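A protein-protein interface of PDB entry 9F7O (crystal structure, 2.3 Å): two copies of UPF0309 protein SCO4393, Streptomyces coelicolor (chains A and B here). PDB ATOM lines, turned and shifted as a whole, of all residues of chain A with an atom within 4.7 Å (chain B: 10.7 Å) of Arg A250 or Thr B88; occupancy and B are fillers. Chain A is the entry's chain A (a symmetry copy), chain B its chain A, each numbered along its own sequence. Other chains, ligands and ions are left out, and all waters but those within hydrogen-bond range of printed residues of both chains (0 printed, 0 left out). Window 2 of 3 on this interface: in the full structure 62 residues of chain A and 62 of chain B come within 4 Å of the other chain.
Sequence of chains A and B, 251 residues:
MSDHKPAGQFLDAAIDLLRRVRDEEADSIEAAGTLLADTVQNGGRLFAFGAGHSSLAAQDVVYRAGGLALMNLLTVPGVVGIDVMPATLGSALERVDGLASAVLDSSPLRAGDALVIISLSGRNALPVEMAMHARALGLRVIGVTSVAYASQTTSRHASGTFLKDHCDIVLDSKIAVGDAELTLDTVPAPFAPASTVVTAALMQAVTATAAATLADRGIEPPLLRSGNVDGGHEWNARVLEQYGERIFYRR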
ATOM      1  N   TYR A  63     -20.123 -11.170 -19.860  1.00  0.00           N
ATOM      2  CA  TYR A  63     -20.002 -11.331 -21.307  1.00  0.00           C
ATOM      3  C   TYR A  63     -18.879 -12.316 -21.619  1.00  0.00           C
ATOM      4  O   TYR A  63     -17.890 -12.003 -22.279  1.00  0.00           O
ATOM      5  CB  TYR A  63     -19.778  -9.979 -21.998  1.00  0.00           C
ATOM      6  CG  TYR A  63     -19.878 -10.067 -23.513  1.00  0.00           C
ATOM      7  CD1 TYR A  63     -21.019 -10.601 -24.127  1.00  0.00           C
ATOM      8  CD2 TYR A  63     -18.834  -9.660 -24.335  1.00  0.00           C
ATOM      9  CE1 TYR A  63     -21.109 -10.722 -25.493  1.00  0.00           C
ATOM     10  CE2 TYR A  63     -18.931  -9.774 -25.698  1.00  0.00           C
ATOM     11  CZ  TYR A  63     -20.060 -10.304 -26.265  1.00  0.00           C
ATOM     12  OH  TYR A  63     -20.173 -10.417 -27.622  1.00  0.00           O
ATOM     13  N   LEU A 240     -30.560 -13.023 -25.725  1.00  0.00           N
ATOM     14  CA  LEU A 240     -30.754 -11.587 -25.562  1.00  0.00           C
ATOM     15  C   LEU A 240     -32.217 -11.212 -25.784  1.00  0.00           C
ATOM     16  O   LEU A 240     -32.787 -10.430 -25.016  1.00  0.00           O
ATOM     17  CB  LEU A 240     -29.846 -10.817 -26.519  1.00  0.00           C
ATOM     18  CG  LEU A 240     -29.981  -9.299 -26.399  1.00  0.00           C
ATOM     19  CD1 LEU A 240     -29.498  -8.762 -25.062  1.00  0.00           C
ATOM     20  CD2 LEU A 240     -29.226  -8.601 -27.564  1.00  0.00           C
ATOM     21  N   ILE A 247     -30.355  -7.699 -19.249  1.00  0.00           N
ATOM     22  CA  ILE A 247     -28.977  -7.614 -19.729  1.00  0.00           C
ATOM     23  C   ILE A 247     -28.661  -6.146 -19.985  1.00  0.00           C
ATOM     24  O   ILE A 247     -29.359  -5.476 -20.755  1.00  0.00           O
ATOM     25  CB  ILE A 247     -28.752  -8.466 -20.991  1.00  0.00           C
ATOM     26  CG1 ILE A 247     -28.953  -9.946 -20.639  1.00  0.00           C
ATOM     27  CG2 ILE A 247     -27.353  -8.193 -21.531  1.00  0.00           C
ATOM     28  CD1 ILE A 247     -29.110 -10.872 -21.845  1.00  0.00           C
ATOM     29  N   PHE A 248     -27.623  -5.634 -19.326  1.00  0.00           N
ATOM     30  CA  PHE A 248     -27.337  -4.206 -19.358  1.00  0.00           C
ATOM     31  C   PHE A 248     -26.018  -3.834 -20.016  1.00  0.00           C
ATOM     32  O   PHE A 248     -25.728  -2.641 -20.154  1.00  0.00           O
ATOM     33  CB  PHE A 248     -27.394  -3.657 -17.929  1.00  0.00           C
ATOM     34  CG  PHE A 248     -28.736  -3.868 -17.286  1.00  0.00           C
ATOM     35  CD1 PHE A 248     -29.777  -3.004 -17.559  1.00  0.00           C
ATOM     36  CD2 PHE A 248     -28.976  -4.955 -16.458  1.00  0.00           C
ATOM     37  CE1 PHE A 248     -31.028  -3.201 -17.000  1.00  0.00           C
ATOM     38  CE2 PHE A 248     -30.232  -5.161 -15.886  1.00  0.00           C
ATOM     39  CZ  PHE A 248     -31.253  -4.283 -16.148  1.00  0.00           C
ATOM     40  N   TYR A 249     -25.237  -4.801 -20.469  1.00  0.00           N
ATOM     41  CA  TYR A 249     -24.018  -4.499 -21.208  1.00  0.00           C
ATOM     42  C   TYR A 249     -24.230  -4.424 -22.718  1.00  0.00           C
ATOM     43  O   TYR A 249     -23.261  -4.192 -23.449  1.00  0.00           O
ATOM     44  CB  TYR A 249     -22.938  -5.532 -20.889  1.00  0.00           C
ATOM     45  CG  TYR A 249     -23.379  -6.969 -21.079  1.00  0.00           C
ATOM     46  CD1 TYR A 249     -23.457  -7.534 -22.336  1.00  0.00           C
ATOM     47  CD2 TYR A 249     -23.705  -7.763 -19.991  1.00  0.00           C
ATOM     48  CE1 TYR A 249     -23.858  -8.848 -22.499  1.00  0.00           C
ATOM     49  CE2 TYR A 249     -24.104  -9.060 -20.151  1.00  0.00           C
ATOM     50  CZ  TYR A 249     -24.187  -9.599 -21.398  1.00  0.00           C
ATOM     51  OH  TYR A 249     -24.595 -10.911 -21.543  1.00  0.00           O
ATOM     52  N   ARG A 250     -25.460  -4.569 -23.197  1.00  0.00           N
ATOM     53  CA  ARG A 250     -25.760  -4.406 -24.615  1.00  0.00           C
ATOM     54  C   ARG A 250     -27.262  -4.213 -24.755  1.00  0.00           C
ATOM     55  O   ARG A 250     -28.019  -4.394 -23.795  1.00  0.00           O
ATOM     56  CB  ARG A 250     -25.291  -5.613 -25.429  1.00  0.00           C
ATOM     57  CG  ARG A 250     -26.079  -6.858 -25.088  1.00  0.00           C
ATOM     58  CD  ARG A 250     -25.482  -8.126 -25.657  1.00  0.00           C
ATOM     59  NE  ARG A 250     -25.521  -8.129 -27.113  1.00  0.00           N
ATOM     60  CZ  ARG A 250     -25.151  -9.155 -27.870  1.00  0.00           C
ATOM     61  NH1 ARG A 250     -24.804 -10.317 -27.338  1.00  0.00           N
ATOM     62  NH2 ARG A 250     -25.130  -9.009 -29.194  1.00  0.00           N
ATOM     63  N   ARG A 251     -27.687  -3.868 -25.971  1.00  0.00           N
ATOM     64  CA  ARG A 251     -29.107  -3.677 -26.274  1.00  0.00           C
ATOM     65  C   ARG A 251     -29.500  -4.322 -27.601  1.00  0.00           C
ATOM     66  O   ARG A 251     -28.649  -4.530 -28.469  1.00  0.00           O
ATOM     67  CB  ARG A 251     -29.448  -2.189 -26.313  1.00  0.00           C
ATOM     68  CG  ARG A 251     -29.242  -1.437 -25.008  1.00  0.00           C
ATOM     69  CD  ARG A 251     -30.406  -1.684 -24.047  1.00  0.00           C
ATOM     70  NE  ARG A 251     -31.654  -1.100 -24.527  1.00  0.00           N
ATOM     71  CZ  ARG A 251     -32.062   0.132 -24.248  1.00  0.00           C
ATOM     72  NH1 ARG A 251     -31.325   0.961 -23.520  1.00  0.00           N
ATOM     73  NH2 ARG A 251     -33.240   0.542 -24.708  1.00  0.00           N
ATOM     74  N   GLY B  52      -9.697  -7.578 -23.712  1.00  0.00           N
ATOM     75  CA  GLY B  52     -10.883  -8.173 -23.111  1.00  0.00           C
ATOM     76  C   GLY B  52     -10.530  -8.963 -21.860  1.00  0.00           C
ATOM     77  O   GLY B  52      -9.865  -8.456 -20.964  1.00  0.00           O
ATOM     78  N   HIS B  53     -10.993 -10.211 -21.768  1.00  0.00           N
ATOM     79  CA  HIS B  53     -10.707 -11.011 -20.583  1.00  0.00           C
ATOM     80  C   HIS B  53      -9.235 -11.387 -20.492  1.00  0.00           C
ATOM     81  O   HIS B  53      -8.747 -11.652 -19.389  1.00  0.00           O
ATOM     82  CB  HIS B  53     -11.617 -12.240 -20.573  1.00  0.00           C
ATOM     83  CG  HIS B  53     -13.081 -11.895 -20.499  1.00  0.00           C
ATOM     84  ND1 HIS B  53     -13.687 -11.395 -19.358  1.00  0.00           N
ATOM     85  CD2 HIS B  53     -14.052 -11.958 -21.437  1.00  0.00           C
ATOM     86  CE1 HIS B  53     -14.968 -11.172 -19.603  1.00  0.00           C
ATOM     87  NE2 HIS B  53     -15.214 -11.507 -20.858  1.00  0.00           N
ATOM     88  N   GLY B  78     -11.232   0.506 -25.022  1.00  0.00           N
ATOM     89  CA  GLY B  78     -12.282  -0.368 -25.456  1.00  0.00           C
ATOM     90  C   GLY B  78     -12.061  -1.834 -25.159  1.00  0.00           C
ATOM     91  O   GLY B  78     -13.036  -2.597 -25.153  1.00  0.00           O
ATOM     92  N   VAL B  79     -10.813  -2.259 -24.958  1.00  0.00           N
ATOM     93  CA  VAL B  79     -10.554  -3.656 -24.646  1.00  0.00           C
ATOM     94  C   VAL B  79      -9.805  -3.811 -23.325  1.00  0.00           C
ATOM     95  O   VAL B  79      -9.187  -4.837 -23.088  1.00  0.00           O
ATOM     96  CB  VAL B  79      -9.797  -4.355 -25.793  1.00  0.00           C
ATOM     97  CG1 VAL B  79     -10.544  -4.223 -27.093  1.00  0.00           C
ATOM     98  CG2 VAL B  79      -8.398  -3.801 -25.938  1.00  0.00           C
ATOM     99  N   GLY B  81     -10.241  -4.942 -20.087  1.00  0.00           N
ATOM    100  CA  GLY B  81     -11.354  -5.705 -19.507  1.00  0.00           C
ATOM    101  C   GLY B  81     -12.574  -5.653 -20.416  1.00  0.00           C
ATOM    102  O   GLY B  81     -12.482  -5.368 -21.610  1.00  0.00           O
ATOM    103  N   ILE B  82     -13.738  -5.955 -19.840  1.00  0.00           N
ATOM    104  CA  ILE B  82     -15.014  -5.850 -20.557  1.00  0.00           C
ATOM    105  C   ILE B  82     -15.683  -4.528 -20.192  1.00  0.00           C
ATOM    106  O   ILE B  82     -16.910  -4.384 -20.234  1.00  0.00           O
ATOM    107  CB  ILE B  82     -15.907  -7.058 -20.247  1.00  0.00           C
ATOM    108  CG1 ILE B  82     -15.914  -7.345 -18.754  1.00  0.00           C
ATOM    109  CG2 ILE B  82     -15.393  -8.289 -21.003  1.00  0.00           C
ATOM    110  CD1 ILE B  82     -16.778  -6.375 -17.991  1.00  0.00           C
ATOM    111  N   ASP B  83     -14.858  -3.557 -19.813  1.00  0.00           N
ATOM    112  CA  ASP B  83     -15.302  -2.217 -19.435  1.00  0.00           C
ATOM    113  C   ASP B  83     -15.499  -1.396 -20.711  1.00  0.00           C
ATOM    114  O   ASP B  83     -14.662  -0.579 -21.114  1.00  0.00           O
ATOM    115  CB  ASP B  83     -14.274  -1.585 -18.497  1.00  0.00           C
ATOM    116  CG  ASP B  83     -14.756  -0.295 -17.885  1.00  0.00           C
ATOM    117  OD1 ASP B  83     -15.978  -0.167 -17.664  1.00  0.00           O
ATOM    118  OD2 ASP B  83     -13.906   0.584 -17.607  1.00  0.00           O
ATOM    119  N   VAL B  84     -16.626  -1.647 -21.373  1.00  0.00           N
ATOM    120  CA  VAL B  84     -16.957  -0.912 -22.584  1.00  0.00           C
ATOM    121  C   VAL B  84     -18.422  -1.121 -22.927  1.00  0.00           C
ATOM    122  O   VAL B  84     -18.968  -2.211 -22.712  1.00  0.00           O
ATOM    123  CB  VAL B  84     -16.043  -1.353 -23.738  1.00  0.00           C
ATOM    124  CG1 VAL B  84     -16.282  -2.834 -24.095  1.00  0.00           C
ATOM    125  CG2 VAL B  84     -16.269  -0.505 -24.965  1.00  0.00           C
ATOM    126  N   MET B  85     -19.076  -0.073 -23.440  1.00  0.00           N
ATOM    127  CA  MET B  85     -20.482  -0.149 -23.829  1.00  0.00           C
ATOM    128  C   MET B  85     -20.635   0.040 -25.334  1.00  0.00           C
ATOM    129  O   MET B  85     -20.151   1.047 -25.887  1.00  0.00           O
ATOM    130  CB  MET B  85     -21.297   0.902 -23.066  1.00  0.00           C
ATOM    131  CG  MET B  85     -22.775   0.926 -23.400  1.00  0.00           C
ATOM    132  SD  MET B  85     -23.652  -0.539 -22.771  1.00  0.00           S
ATOM    133  CE  MET B  85     -22.689  -0.889 -21.300  1.00  0.00           C
ATOM    134  N   PRO B  86     -21.269  -0.910 -26.043  1.00  0.00           N
ATOM    135  CA  PRO B  86     -21.737  -2.237 -25.584  1.00  0.00           C
ATOM    136  C   PRO B  86     -20.532  -3.186 -25.429  1.00  0.00           C
ATOM    137  O   PRO B  86     -19.482  -2.928 -26.021  1.00  0.00           O
ATOM    138  CB  PRO B  86     -22.712  -2.658 -26.702  1.00  0.00           C
ATOM    139  CG  PRO B  86     -22.101  -2.055 -27.940  1.00  0.00           C
ATOM    140  CD  PRO B  86     -21.481  -0.733 -27.492  1.00  0.00           C
ATOM    141  N   ALA B  87     -20.646  -4.279 -24.667  1.00  0.00           N
ATOM    142  CA  ALA B  87     -19.511  -5.172 -24.481  1.00  0.00           C
ATOM    143  C   ALA B  87     -19.123  -5.858 -25.784  1.00  0.00           C
ATOM    144  O   ALA B  87     -17.979  -6.297 -25.946  1.00  0.00           O
ATOM    145  CB  ALA B  87     -19.838  -6.213 -23.406  1.00  0.00           C
ATOM    146  N   THR B  88     -20.077  -6.002 -26.695  1.00  0.00           N
ATOM    147  CA  THR B  88     -19.794  -6.579 -27.996  1.00  0.00           C
ATOM    148  C   THR B  88     -18.771  -5.759 -28.775  1.00  0.00           C
ATOM    149  O   THR B  88     -18.098  -6.299 -29.665  1.00  0.00           O
ATOM    150  CB  THR B  88     -21.099  -6.672 -28.787  1.00  0.00           C
ATOM    151  OG1 THR B  88     -21.772  -5.406 -28.721  1.00  0.00           O
ATOM    152  CG2 THR B  88     -22.030  -7.737 -28.211  1.00  0.00           C
ATOM    153  N   LEU B  89     -18.671  -4.449 -28.505  1.00  0.00           N
ATOM    154  CA  LEU B  89     -17.681  -3.640 -29.210  1.00  0.00           C
ATOM    155  C   LEU B  89     -16.267  -4.146 -28.942  1.00  0.00           C
ATOM    156  O   LEU B  89     -15.411  -4.134 -29.836  1.00  0.00           O
ATOM    157  CB  LEU B  89     -17.808  -2.177 -28.798  1.00  0.00           C
ATOM    158  CG  LEU B  89     -16.844  -1.219 -29.501  1.00  0.00           C
ATOM    159  CD1 LEU B  89     -16.903  -1.287 -30.996  1.00  0.00           C
ATOM    160  CD2 LEU B  89     -17.151   0.234 -28.998  1.00  0.00           C
ATOM    161  N   GLY B  90     -16.014  -4.603 -27.717  1.00  0.00           N
ATOM    162  CA  GLY B  90     -14.697  -5.104 -27.380  1.00  0.00           C
ATOM    163  C   GLY B  90     -14.267  -6.221 -28.297  1.00  0.00           C
ATOM    164  O   GLY B  90     -13.105  -6.287 -28.704  1.00  0.00           O
ATOM    165  N   SER B  91     -15.195  -7.126 -28.625  1.00  0.00           N
ATOM    166  CA  SER B  91     -14.852  -8.204 -29.549  1.00  0.00           C
ATOM    167  C   SER B  91     -14.579  -7.663 -30.943  1.00  0.00           C
ATOM    168  O   SER B  91     -13.665  -8.131 -31.621  1.00  0.00           O
ATOM    169  CB  SER B  91     -15.955  -9.248 -29.630  1.00  0.00           C
ATOM    170  OG  SER B  91     -16.313  -9.644 -28.333  1.00  0.00           O
ATOM    171  N   ALA B  92     -15.356  -6.677 -31.390  1.00  0.00           N
ATOM    172  CA  ALA B  92     -15.129  -6.105 -32.715  1.00  0.00           C
ATOM    173  C   ALA B  92     -13.768  -5.427 -32.796  1.00  0.00           C
ATOM    174  O   ALA B  92     -13.100  -5.471 -33.839  1.00  0.00           O
ATOM    175  CB  ALA B  92     -16.239  -5.111 -33.072  1.00  0.00           C
ATOM    176  N   LEU B  93     -13.333  -4.800 -31.704  1.00  0.00           N
ATOM    177  CA  LEU B  93     -12.099  -4.030 -31.754  1.00  0.00           C
ATOM    178  C   LEU B  93     -10.895  -4.924 -31.948  1.00  0.00           C
ATOM    179  O   LEU B  93      -9.912  -4.497 -32.558  1.00  0.00           O
ATOM    180  CB  LEU B  93     -11.935  -3.200 -30.487  1.00  0.00           C
ATOM    181  CG  LEU B  93     -12.858  -1.999 -30.345  1.00  0.00           C
ATOM    182  CD1 LEU B  93     -12.733  -1.502 -28.909  1.00  0.00           C
ATOM    183  CD2 LEU B  93     -12.500  -0.908 -31.301  1.00  0.00           C
ATOM    184  N   GLU B  94     -10.950  -6.165 -31.460  1.00  0.00           N
ATOM    185  CA  GLU B  94      -9.828  -7.092 -31.640  1.00  0.00           C
ATOM    186  C   GLU B  94      -9.491  -7.343 -33.114  1.00  0.00           C
ATOM    187  O   GLU B  94      -8.429  -7.901 -33.416  1.00  0.00           O
ATOM    188  CB  GLU B  94     -10.121  -8.445 -30.975  1.00  0.00           C
ATOM    189  CG  GLU B  94     -10.337  -8.378 -29.470  1.00  0.00           C
ATOM    190  CD  GLU B  94     -10.722  -9.719 -28.878  1.00  0.00           C
ATOM    191  OE1 GLU B  94     -10.627 -10.723 -29.617  1.00  0.00           O
ATOM    192  OE2 GLU B  94     -11.117  -9.763 -27.683  1.00  0.00           O
ATOM    193  N   ARG B  95     -10.376  -6.976 -34.036  1.00  0.00           N
ATOM    194  CA  ARG B  95     -10.177  -7.241 -35.451  1.00  0.00           C
ATOM    195  C   ARG B  95      -9.851  -5.976 -36.230  1.00  0.00           C
ATOM    196  O   ARG B  95      -9.735  -6.026 -37.452  1.00  0.00           O
ATOM    197  CB  ARG B  95     -11.414  -7.933 -36.027  1.00  0.00           C
ATOM    198  CG  ARG B  95     -11.901  -9.066 -35.151  1.00  0.00           C
ATOM    199  CD  ARG B  95     -12.746 -10.055 -35.929  1.00  0.00           C
ATOM    200  NE  ARG B  95     -13.102 -11.219 -35.124  1.00  0.00           N
ATOM    201  CZ  ARG B  95     -13.788 -12.259 -35.580  1.00  0.00           C
ATOM    202  NH1 ARG B  95     -14.185 -12.328 -36.841  1.00  0.00           N
ATOM    203  NH2 ARG B  95     -14.079 -13.257 -34.749  1.00  0.00           N
ATOM    204  N   VAL B  96      -9.643  -4.860 -35.542  1.00  0.00           N
ATOM    205  CA  VAL B  96      -9.375  -3.583 -36.191  1.00  0.00           C
ATOM    206  C   VAL B  96      -7.879  -3.495 -36.460  1.00  0.00           C
ATOM    207  O   VAL B  96      -7.083  -3.334 -35.533  1.00  0.00           O
ATOM    208  CB  VAL B  96      -9.854  -2.398 -35.342  1.00  0.00           C
ATOM    209  CG1 VAL B  96      -9.306  -1.072 -35.915  1.00  0.00           C
ATOM    210  CG2 VAL B  96     -11.386  -2.340 -35.293  1.00  0.00           C
ATOM    211  N   ASN B 124      -6.258 -13.131 -33.558  1.00  0.00           N
ATOM    212  CA  ASN B 124      -6.940 -11.930 -34.002  1.00  0.00           C
ATOM    213  C   ASN B 124      -5.948 -10.848 -34.425  1.00  0.00           C
ATOM    214  O   ASN B 124      -4.766 -10.863 -34.070  1.00  0.00           O
ATOM    215  CB  ASN B 124      -7.868 -11.415 -32.906  1.00  0.00           C
ATOM    216  CG  ASN B 124      -9.154 -12.220 -32.810  1.00  0.00           C
ATOM    217  OD1 ASN B 124      -9.715 -12.627 -33.826  1.00  0.00           O
ATOM    218  ND2 ASN B 124      -9.636 -12.430 -31.586  1.00  0.00           N
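Hydrophobic or aromatic side chains of chain A within 4 Å of the printed part of chain B: Tyr A63 and Tyr A249. Of the 21 printed residues of chain B, 6 touch a printed residue of chain A. Printed residues of chain B that touch a printed residue of chain A: His B53, Met B85, Pro B86, Ala B87, Thr B88 and Ser B91. Hydrophobic or aromatic side chains of chain B within 4 Å of the printed part of chain A: His B53, Met B85, Pro B86 and Ala B87. Among the printed residues, 9 pairs touch across the chains. Among the printed residues, no Asp or Glu carboxylate lies within 4 Å of a Lys or Arg side-chain nitrogen of the other chain.
Among the printed residues, pairs that only touch across the chains: Tyr A249 with Pro B86 (3.3 Å), Tyr A63 with Thr B88 (3.3 Å), Arg A250 with Thr B88 (3.4 Å), Tyr A63 with Ala B87 (3.6 Å), Phe A248 with Met B85 (3.7 Å) and Tyr A63 with Ser B91 (3.7 Å).
Arg A250 touches just one residue of chain B: Thr B88. Of chain A, only Tyr A63 (3.3 Å) and Arg A250 (3.4 Å) come within 4 Å of Thr B88. Of chain B, only Met B85, Pro B86 and Ala B87 come within 4 Å of Tyr A249. Of the printed residues of chain A, Met B85 touches Phe A248 (3.7 Å) and Tyr A249 (3.7 Å). Of the printed residues of chain A, Pro B86 touches Tyr A249 (3.3 Å). Gly B78 touches none of the printed residues of chain A. The nearest residue of chain B that does not touch Arg A250 is Pro B86 (4.1 Å). The nearest printed residue of chain A that does not touch Thr B88 is Tyr A249 (4.9 Å).
A ring nitrogen (NE2) of His B53 sits at hydrogen-bond distance from the backbone carbonyl oxygen (O) of Tyr A63. The backbone carbonyl oxygen (O) of Tyr A249 sits at hydrogen-bond distance from the backbone NH (N) of Ala B87, 2.9 Å away. SD of Met B85 lies close to O of Tyr A249 (3.7 Å).
No position is printed for both chains.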
